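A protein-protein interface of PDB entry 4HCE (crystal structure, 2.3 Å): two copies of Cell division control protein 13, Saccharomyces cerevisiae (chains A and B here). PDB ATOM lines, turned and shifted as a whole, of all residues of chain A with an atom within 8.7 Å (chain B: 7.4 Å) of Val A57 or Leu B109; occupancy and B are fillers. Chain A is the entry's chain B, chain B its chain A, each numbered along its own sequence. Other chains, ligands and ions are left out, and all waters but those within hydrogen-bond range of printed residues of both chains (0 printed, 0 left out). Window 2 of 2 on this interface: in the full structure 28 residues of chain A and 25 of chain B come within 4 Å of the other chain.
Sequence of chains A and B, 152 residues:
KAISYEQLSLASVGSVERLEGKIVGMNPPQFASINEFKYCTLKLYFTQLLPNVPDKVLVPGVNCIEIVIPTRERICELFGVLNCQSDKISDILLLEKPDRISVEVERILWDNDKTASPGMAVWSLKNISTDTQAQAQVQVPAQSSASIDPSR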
ATOM      1  N   VAL A  24     -30.714  26.315  23.637  1.00  0.00           N
ATOM      2  CA  VAL A  24     -30.208  25.515  22.540  1.00  0.00           C
ATOM      3  C   VAL A  24     -28.682  25.489  22.524  1.00  0.00           C
ATOM      4  O   VAL A  24     -28.095  24.920  21.634  1.00  0.00           O
ATOM      5  CB  VAL A  24     -30.736  26.007  21.173  1.00  0.00           C
ATOM      6  CG1 VAL A  24     -32.220  25.743  21.058  1.00  0.00           C
ATOM      7  CG2 VAL A  24     -30.448  27.492  20.980  1.00  0.00           C
ATOM      8  N   THR A  47     -34.022  30.351  22.229  1.00  0.00           N
ATOM      9  CA  THR A  47     -34.905  30.613  21.087  1.00  0.00           C
ATOM     10  C   THR A  47     -36.196  29.773  21.147  1.00  0.00           C
ATOM     11  O   THR A  47     -36.196  28.651  21.677  1.00  0.00           O
ATOM     12  CB  THR A  47     -34.219  30.382  19.716  1.00  0.00           C
ATOM     13  OG1 THR A  47     -35.065  30.906  18.672  1.00  0.00           O
ATOM     14  CG2 THR A  47     -33.954  28.895  19.454  1.00  0.00           C
ATOM     15  N   LEU A  49     -37.713  29.726  18.046  1.00  0.00           N
ATOM     16  CA  LEU A  49     -37.745  29.588  16.591  1.00  0.00           C
ATOM     17  C   LEU A  49     -36.939  28.381  16.148  1.00  0.00           C
ATOM     18  O   LEU A  49     -35.720  28.402  16.240  1.00  0.00           O
ATOM     19  CB  LEU A  49     -37.115  30.810  15.938  1.00  0.00           C
ATOM     20  CG  LEU A  49     -37.980  31.898  15.338  1.00  0.00           C
ATOM     21  CD1 LEU A  49     -38.344  31.449  13.915  1.00  0.00           C
ATOM     22  CD2 LEU A  49     -39.218  32.235  16.189  1.00  0.00           C
ATOM     23  N   LEU A  50     -37.617  27.347  15.652  1.00  0.00           N
ATOM     24  CA  LEU A  50     -36.950  26.130  15.179  1.00  0.00           C
ATOM     25  C   LEU A  50     -35.790  25.716  16.077  1.00  0.00           C
ATOM     26  O   LEU A  50     -34.680  25.557  15.586  1.00  0.00           O
ATOM     27  CB  LEU A  50     -36.420  26.315  13.751  1.00  0.00           C
ATOM     28  CG  LEU A  50     -37.406  26.683  12.650  1.00  0.00           C
ATOM     29  CD1 LEU A  50     -36.637  27.063  11.391  1.00  0.00           C
ATOM     30  CD2 LEU A  50     -38.417  25.556  12.409  1.00  0.00           C
ATOM     31  N   VAL A  53     -34.200  21.943  14.719  1.00  0.00           N
ATOM     32  CA  VAL A  53     -33.545  21.742  13.440  1.00  0.00           C
ATOM     33  C   VAL A  53     -32.022  21.595  13.557  1.00  0.00           C
ATOM     34  O   VAL A  53     -31.334  22.542  13.937  1.00  0.00           O
ATOM     35  CB  VAL A  53     -33.963  22.841  12.436  1.00  0.00           C
ATOM     36  CG1 VAL A  53     -35.468  23.026  12.492  1.00  0.00           C
ATOM     37  CG2 VAL A  53     -33.285  24.170  12.728  1.00  0.00           C
ATOM     38  N   PRO A  54     -31.498  20.375  13.305  1.00  0.00           N
ATOM     39  CA  PRO A  54     -30.061  20.274  13.054  1.00  0.00           C
ATOM     40  C   PRO A  54     -29.831  20.807  11.645  1.00  0.00           C
ATOM     41  O   PRO A  54     -30.624  20.506  10.750  1.00  0.00           O
ATOM     42  CB  PRO A  54     -29.789  18.766  13.150  1.00  0.00           C
ATOM     43  CG  PRO A  54     -30.938  18.213  13.937  1.00  0.00           C
ATOM     44  CD  PRO A  54     -32.108  19.044  13.500  1.00  0.00           C
ATOM     45  N   ASP A  55     -28.765  21.585  11.460  1.00  0.00           N
ATOM     46  CA  ASP A  55     -28.627  22.542  10.346  1.00  0.00           C
ATOM     47  C   ASP A  55     -28.575  23.961  10.916  1.00  0.00           C
ATOM     48  O   ASP A  55     -27.952  24.848  10.318  1.00  0.00           O
ATOM     49  CB  ASP A  55     -29.760  22.407   9.295  1.00  0.00           C
ATOM     50  CG  ASP A  55     -30.477  23.741   8.989  1.00  0.00           C
ATOM     51  OD1 ASP A  55     -29.853  24.671   8.430  1.00  0.00           O
ATOM     52  OD2 ASP A  55     -31.686  23.852   9.291  1.00  0.00           O
ATOM     53  N   LYS A  56     -29.227  24.160  12.070  1.00  0.00           N
ATOM     54  CA  LYS A  56     -29.351  25.487  12.670  1.00  0.00           C
ATOM     55  C   LYS A  56     -28.003  26.134  12.937  1.00  0.00           C
ATOM     56  O   LYS A  56     -27.123  25.565  13.583  1.00  0.00           O
ATOM     57  CB  LYS A  56     -30.213  25.480  13.944  1.00  0.00           C
ATOM     58  CG  LYS A  56     -29.531  25.006  15.223  1.00  0.00           C
ATOM     59  CD  LYS A  56     -30.293  25.491  16.452  1.00  0.00           C
ATOM     60  CE  LYS A  56     -30.027  24.631  17.677  1.00  0.00           C
ATOM     61  NZ  LYS A  56     -30.798  23.355  17.653  1.00  0.00           N
ATOM     62  N   VAL A  57     -27.843  27.321  12.373  1.00  0.00           N
ATOM     63  CA  VAL A  57     -26.734  28.168  12.722  1.00  0.00           C
ATOM     64  C   VAL A  57     -27.303  29.273  13.611  1.00  0.00           C
ATOM     65  O   VAL A  57     -28.154  30.056  13.187  1.00  0.00           O
ATOM     66  CB  VAL A  57     -26.065  28.769  11.474  1.00  0.00           C
ATOM     67  CG1 VAL A  57     -24.994  29.764  11.885  1.00  0.00           C
ATOM     68  CG2 VAL A  57     -25.504  27.670  10.566  1.00  0.00           C
ATOM     69  N   LEU A  58     -26.829  29.326  14.845  1.00  0.00           N
ATOM     70  CA  LEU A  58     -27.273  30.346  15.771  1.00  0.00           C
ATOM     71  C   LEU A  58     -26.680  31.682  15.371  1.00  0.00           C
ATOM     72  O   LEU A  58     -25.497  31.761  15.002  1.00  0.00           O
ATOM     73  CB  LEU A  58     -26.838  29.998  17.196  1.00  0.00           C
ATOM     74  CG  LEU A  58     -27.441  28.760  17.854  1.00  0.00           C
ATOM     75  CD1 LEU A  58     -26.990  28.672  19.307  1.00  0.00           C
ATOM     76  CD2 LEU A  58     -28.953  28.847  17.746  1.00  0.00           C
ATOM     77  N   VAL A  59     -27.494  32.722  15.432  1.00  0.00           N
ATOM     78  CA  VAL A  59     -26.988  34.080  15.335  1.00  0.00           C
ATOM     79  C   VAL A  59     -27.690  34.942  16.388  1.00  0.00           C
ATOM     80  O   VAL A  59     -28.844  35.342  16.216  1.00  0.00           O
ATOM     81  CB  VAL A  59     -26.916  34.611  13.850  1.00  0.00           C
ATOM     82  CG1 VAL A  59     -27.993  34.025  12.951  1.00  0.00           C
ATOM     83  CG2 VAL A  59     -26.845  36.120  13.743  1.00  0.00           C
ATOM     84  N   PRO A  60     -27.019  35.125  17.549  1.00  0.00           N
ATOM     85  CA  PRO A  60     -27.500  35.927  18.685  1.00  0.00           C
ATOM     86  C   PRO A  60     -27.922  37.309  18.234  1.00  0.00           C
ATOM     87  O   PRO A  60     -27.180  37.988  17.517  1.00  0.00           O
ATOM     88  CB  PRO A  60     -26.272  36.048  19.586  1.00  0.00           C
ATOM     89  CG  PRO A  60     -25.432  34.848  19.261  1.00  0.00           C
ATOM     90  CD  PRO A  60     -25.736  34.450  17.843  1.00  0.00           C
ATOM     91  N   VAL A  62     -30.427  37.870  16.203  1.00  0.00           N
ATOM     92  CA  VAL A  62     -31.356  37.730  15.080  1.00  0.00           C
ATOM     93  C   VAL A  62     -32.197  36.463  15.167  1.00  0.00           C
ATOM     94  O   VAL A  62     -33.356  36.461  14.799  1.00  0.00           O
ATOM     95  CB  VAL A  62     -30.683  37.968  13.680  1.00  0.00           C
ATOM     96  CG1 VAL A  62     -29.210  38.273  13.793  1.00  0.00           C
ATOM     97  CG2 VAL A  62     -30.970  36.867  12.663  1.00  0.00           C
ATOM     98  N   ASN A  63     -31.622  35.434  15.764  1.00  0.00           N
ATOM     99  CA  ASN A  63     -32.101  34.065  15.693  1.00  0.00           C
ATOM    100  C   ASN A  63     -32.507  33.539  17.044  1.00  0.00           C
ATOM    101  O   ASN A  63     -33.238  32.570  17.155  1.00  0.00           O
ATOM    102  CB  ASN A  63     -30.891  33.198  15.333  1.00  0.00           C
ATOM    103  CG  ASN A  63     -31.248  32.173  14.362  1.00  0.00           C
ATOM    104  OD1 ASN A  63     -32.370  32.189  13.876  1.00  0.00           O
ATOM    105  ND2 ASN A  63     -30.345  31.299  14.050  1.00  0.00           N
ATOM    106  N   CYS A  64     -31.917  34.153  18.062  1.00  0.00           N
ATOM    107  CA  CYS A  64     -31.936  33.680  19.412  1.00  0.00           C
ATOM    108  C   CYS A  64     -31.422  34.854  20.206  1.00  0.00           C
ATOM    109  O   CYS A  64     -30.962  35.844  19.633  1.00  0.00           O
ATOM    110  CB  CYS A  64     -31.000  32.475  19.566  1.00  0.00           C
ATOM    111  SG  CYS A  64     -29.234  32.757  19.202  1.00  0.00           S
ATOM    112  N   VAL B  13     -22.315  33.598   5.710  1.00  0.00           N
ATOM    113  CA  VAL B  13     -21.035  32.988   6.010  1.00  0.00           C
ATOM    114  C   VAL B  13     -20.143  33.014   4.761  1.00  0.00           C
ATOM    115  O   VAL B  13     -20.572  32.653   3.659  1.00  0.00           O
ATOM    116  CB  VAL B  13     -21.219  31.541   6.520  1.00  0.00           C
ATOM    117  CG1 VAL B  13     -19.883  30.803   6.582  1.00  0.00           C
ATOM    118  CG2 VAL B  13     -21.898  31.544   7.884  1.00  0.00           C
ATOM    119  N   GLY B  14     -18.902  33.454   4.931  1.00  0.00           N
ATOM    120  CA  GLY B  14     -17.983  33.523   3.813  1.00  0.00           C
ATOM    121  C   GLY B  14     -17.764  34.957   3.397  1.00  0.00           C
ATOM    122  O   GLY B  14     -16.759  35.243   2.754  1.00  0.00           O
ATOM    123  N   GLU B 106     -14.048  38.273   8.499  1.00  0.00           N
ATOM    124  CA  GLU B 106     -14.691  37.194   7.748  1.00  0.00           C
ATOM    125  C   GLU B 106     -15.855  36.600   8.566  1.00  0.00           C
ATOM    126  O   GLU B 106     -15.699  36.331   9.758  1.00  0.00           O
ATOM    127  CB  GLU B 106     -13.651  36.113   7.398  1.00  0.00           C
ATOM    128  CG  GLU B 106     -14.162  35.017   6.471  1.00  0.00           C
ATOM    129  CD  GLU B 106     -13.140  33.917   6.208  1.00  0.00           C
ATOM    130  OE1 GLU B 106     -13.496  32.955   5.506  1.00  0.00           O
ATOM    131  OE2 GLU B 106     -11.989  33.999   6.698  1.00  0.00           O
ATOM    132  N   ARG B 107     -17.016  36.443   7.933  1.00  0.00           N
ATOM    133  CA  ARG B 107     -18.144  35.717   8.519  1.00  0.00           C
ATOM    134  C   ARG B 107     -17.838  34.241   8.464  1.00  0.00           C
ATOM    135  O   ARG B 107     -17.751  33.667   7.365  1.00  0.00           O
ATOM    136  CB  ARG B 107     -19.443  35.936   7.723  1.00  0.00           C
ATOM    137  CG  ARG B 107     -20.429  36.921   8.290  1.00  0.00           C
ATOM    138  CD  ARG B 107     -21.487  36.325   9.202  1.00  0.00           C
ATOM    139  NE  ARG B 107     -21.301  36.884  10.527  1.00  0.00           N
ATOM    140  CZ  ARG B 107     -22.250  37.168  11.416  1.00  0.00           C
ATOM    141  NH1 ARG B 107     -23.530  36.968  11.172  1.00  0.00           N
ATOM    142  NH2 ARG B 107     -21.884  37.677  12.580  1.00  0.00           N
ATOM    143  N   ILE B 108     -17.713  33.628   9.637  1.00  0.00           N
ATOM    144  CA  ILE B 108     -17.395  32.205   9.724  1.00  0.00           C
ATOM    145  C   ILE B 108     -18.476  31.441  10.469  1.00  0.00           C
ATOM    146  O   ILE B 108     -19.198  31.988  11.318  1.00  0.00           O
ATOM    147  CB  ILE B 108     -16.027  31.918  10.393  1.00  0.00           C
ATOM    148  CG1 ILE B 108     -16.020  32.434  11.837  1.00  0.00           C
ATOM    149  CG2 ILE B 108     -14.886  32.529   9.578  1.00  0.00           C
ATOM    150  CD1 ILE B 108     -14.969  31.806  12.718  1.00  0.00           C
ATOM    151  N   LEU B 109     -18.584  30.167  10.115  1.00  0.00           N
ATOM    152  CA  LEU B 109     -19.388  29.242  10.850  1.00  0.00           C
ATOM    153  C   LEU B 109     -18.493  28.739  11.956  1.00  0.00           C
ATOM    154  O   LEU B 109     -17.559  27.993  11.731  1.00  0.00           O
ATOM    155  CB  LEU B 109     -19.858  28.107   9.953  1.00  0.00           C
ATOM    156  CG  LEU B 109     -20.699  27.073  10.687  1.00  0.00           C
ATOM    157  CD1 LEU B 109     -22.000  27.700  11.178  1.00  0.00           C
ATOM    158  CD2 LEU B 109     -20.967  25.905   9.759  1.00  0.00           C
ATOM    159  N   TRP B 110     -18.767  29.188  13.162  1.00  0.00           N
ATOM    160  CA  TRP B 110     -17.932  28.839  14.271  1.00  0.00           C
ATOM    161  C   TRP B 110     -18.524  27.667  14.995  1.00  0.00           C
ATOM    162  O   TRP B 110     -19.558  27.777  15.648  1.00  0.00           O
ATOM    163  CB  TRP B 110     -17.771  30.063  15.143  1.00  0.00           C
ATOM    164  CG  TRP B 110     -16.797  29.932  16.269  1.00  0.00           C
ATOM    165  CD1 TRP B 110     -15.596  29.235  16.290  1.00  0.00           C
ATOM    166  CD2 TRP B 110     -16.901  30.564  17.577  1.00  0.00           C
ATOM    167  NE1 TRP B 110     -14.975  29.377  17.497  1.00  0.00           N
ATOM    168  CE2 TRP B 110     -15.709  30.160  18.321  1.00  0.00           C
ATOM    169  CE3 TRP B 110     -17.839  31.387  18.193  1.00  0.00           C
ATOM    170  CZ2 TRP B 110     -15.486  30.575  19.627  1.00  0.00           C
ATOM    171  CZ3 TRP B 110     -17.599  31.808  19.502  1.00  0.00           C
ATOM    172  CH2 TRP B 110     -16.456  31.409  20.202  1.00  0.00           C
ATOM    173  N   ASP B 111     -17.870  26.522  14.821  1.00  0.00           N
ATOM    174  CA  ASP B 111     -18.249  25.243  15.407  1.00  0.00           C
ATOM    175  C   ASP B 111     -16.948  24.492  15.689  1.00  0.00           C
ATOM    176  O   ASP B 111     -16.244  24.135  14.744  1.00  0.00           O
ATOM    177  CB  ASP B 111     -19.108  24.461  14.410  1.00  0.00           C
ATOM    178  CG  ASP B 111     -19.962  23.385  15.070  1.00  0.00           C
ATOM    179  OD1 ASP B 111     -19.605  22.856  16.148  1.00  0.00           O
ATOM    180  OD2 ASP B 111     -21.011  23.056  14.488  1.00  0.00           O
ATOM    181  N   ASN B 112     -16.563  24.259  16.945  1.00  0.00           N
ATOM    182  CA  ASN B 112     -17.214  24.647  18.208  1.00  0.00           C
ATOM    183  C   ASN B 112     -17.206  23.430  19.147  1.00  0.00           C
ATOM    184  O   ASN B 112     -18.089  23.276  20.004  1.00  0.00           O
ATOM    185  CB  ASN B 112     -18.634  25.221  18.031  1.00  0.00           C
ATOM    186  CG  ASN B 112     -19.044  26.138  19.176  1.00  0.00           C
ATOM    187  OD1 ASN B 112     -18.258  26.989  19.629  1.00  0.00           O
ATOM    188  ND2 ASN B 112     -20.281  25.972  19.652  1.00  0.00           N
ATOM    189  N   PRO B 118     -24.506  24.015  18.870  1.00  0.00           N
ATOM    190  CA  PRO B 118     -24.616  24.364  17.466  1.00  0.00           C
ATOM    191  C   PRO B 118     -23.528  25.357  17.098  1.00  0.00           C
ATOM    192  O   PRO B 118     -23.028  26.084  17.966  1.00  0.00           O
ATOM    193  CB  PRO B 118     -26.002  25.028  17.366  1.00  0.00           C
ATOM    194  CG  PRO B 118     -26.549  25.070  18.764  1.00  0.00           C
ATOM    195  CD  PRO B 118     -25.398  24.841  19.697  1.00  0.00           C
ATOM    196  N   GLY B 119     -23.156  25.367  15.821  1.00  0.00           N
ATOM    197  CA  GLY B 119     -22.327  26.422  15.270  1.00  0.00           C
ATOM    198  C   GLY B 119     -23.034  27.771  15.318  1.00  0.00           C
ATOM    199  O   GLY B 119     -24.264  27.858  15.302  1.00  0.00           O
ATOM    200  N   MET B 120     -22.236  28.822  15.406  1.00  0.00           N
ATOM    201  CA  MET B 120     -22.716  30.179  15.348  1.00  0.00           C
ATOM    202  C   MET B 120     -22.018  30.923  14.230  1.00  0.00           C
ATOM    203  O   MET B 120     -20.802  30.755  14.035  1.00  0.00           O
ATOM    204  CB  MET B 120     -22.415  30.883  16.657  1.00  0.00           C
ATOM    205  CG  MET B 120     -23.295  30.447  17.810  1.00  0.00           C
ATOM    206  SD  MET B 120     -22.880  31.383  19.289  1.00  0.00           S
ATOM    207  CE  MET B 120     -21.265  30.677  19.593  1.00  0.00           C
ATOM    208  N   ALA B 121     -22.772  31.743  13.505  1.00  0.00           N
ATOM    209  CA  ALA B 121     -22.175  32.688  12.580  1.00  0.00           C
ATOM    210  C   ALA B 121     -21.565  33.807  13.410  1.00  0.00           C
ATOM    211  O   ALA B 121     -22.243  34.392  14.248  1.00  0.00           O
ATOM    212  CB  ALA B 121     -23.200  33.233  11.595  1.00  0.00           C
ATOM    213  N   VAL B 122     -20.280  34.079  13.195  1.00  0.00           N
ATOM    214  CA  VAL B 122     -19.594  35.169  13.867  1.00  0.00           C
ATOM    215  C   VAL B 122     -18.623  35.890  12.923  1.00  0.00           C
ATOM    216  O   VAL B 122     -18.345  35.408  11.811  1.00  0.00           O
ATOM    217  CB  VAL B 122     -18.825  34.692  15.123  1.00  0.00           C
ATOM    218  CG1 VAL B 122     -19.781  34.316  16.247  1.00  0.00           C
ATOM    219  CG2 VAL B 122     -17.896  33.533  14.791  1.00  0.00           C
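Among the printed residues, pairs that only touch across the chains: Val A24 with Pro B118 (3.3 Å), Lys A56 with Pro B118 (3.7 Å), Val A57 with Leu B109 (3.6 Å), Val A57 with Gly B119 (3.6 Å), Val A57 with Met B120 (3.96 Å), Val A57 with Ala B121 (3.4 Å), Leu A58 with Pro B118 (3.7 Å) and Leu A58 with Met B120 (3.2 Å).
The backbone NH (N) of Leu A58 is in hydrogen-bond range of the backbone carbonyl oxygen (O) of Gly B119, 3.0 Å away. The backbone NH (N) of Ala B121 is in hydrogen-bond range of the backbone carbonyl oxygen (O) of Leu A58, 3.1 Å away.
No position is printed for both chains. Of the 10 pairs that touch across the chains among the printed residues, none has its exchanged pair printed and touching as well.
Hydrophobic or aromatic side chains of chain A within 4 Å of the printed part of chain B: Val A57 and Leu A58. Printed residues of chain B that touch a printed residue of chain A: Leu B109, Pro B118, Gly B119, Met B120 and Ala B121. Hydrophobic or aromatic side chains of chain B that line the printed part of chain A: Leu B109, Pro B118, Met B120 and Ala B121. Among the printed residues, no Asp or Glu carboxylate lies within 4 Å of a Lys or Arg side-chain nitrogen of the other chain.
The backbone NH of Trp B110 lies within hydrogen-bond range of the backbone carbonyl oxygen of Met B120 (2.7 Å). The side-chain carboxylate (OD2) of Asp B111 is in hydrogen-bond range of the backbone NH (N) of Gly B119 (3.4 Å). O of Pro B118 is in hydrogen-bond range of ND2 of Asn B112 (3.2 Å). O of Val A57 is in hydrogen-bond range of ND2 of Asn A63.
Val A57 touches just these residues of chain B: Leu B109, Gly B119, Met B120 and Ala B121. Leu B109 touches just one residue of chain A: Val A57. Of the printed residues of chain A, Ala B121 touches Val A57 (3.4 Å) and Leu A58 (3.1 Å). Printed residues of chain A within 4 Å of Pro B118: Val A24 (3.3 Å), Lys A56 (3.7 Å) and Leu A58 (3.7 Å).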
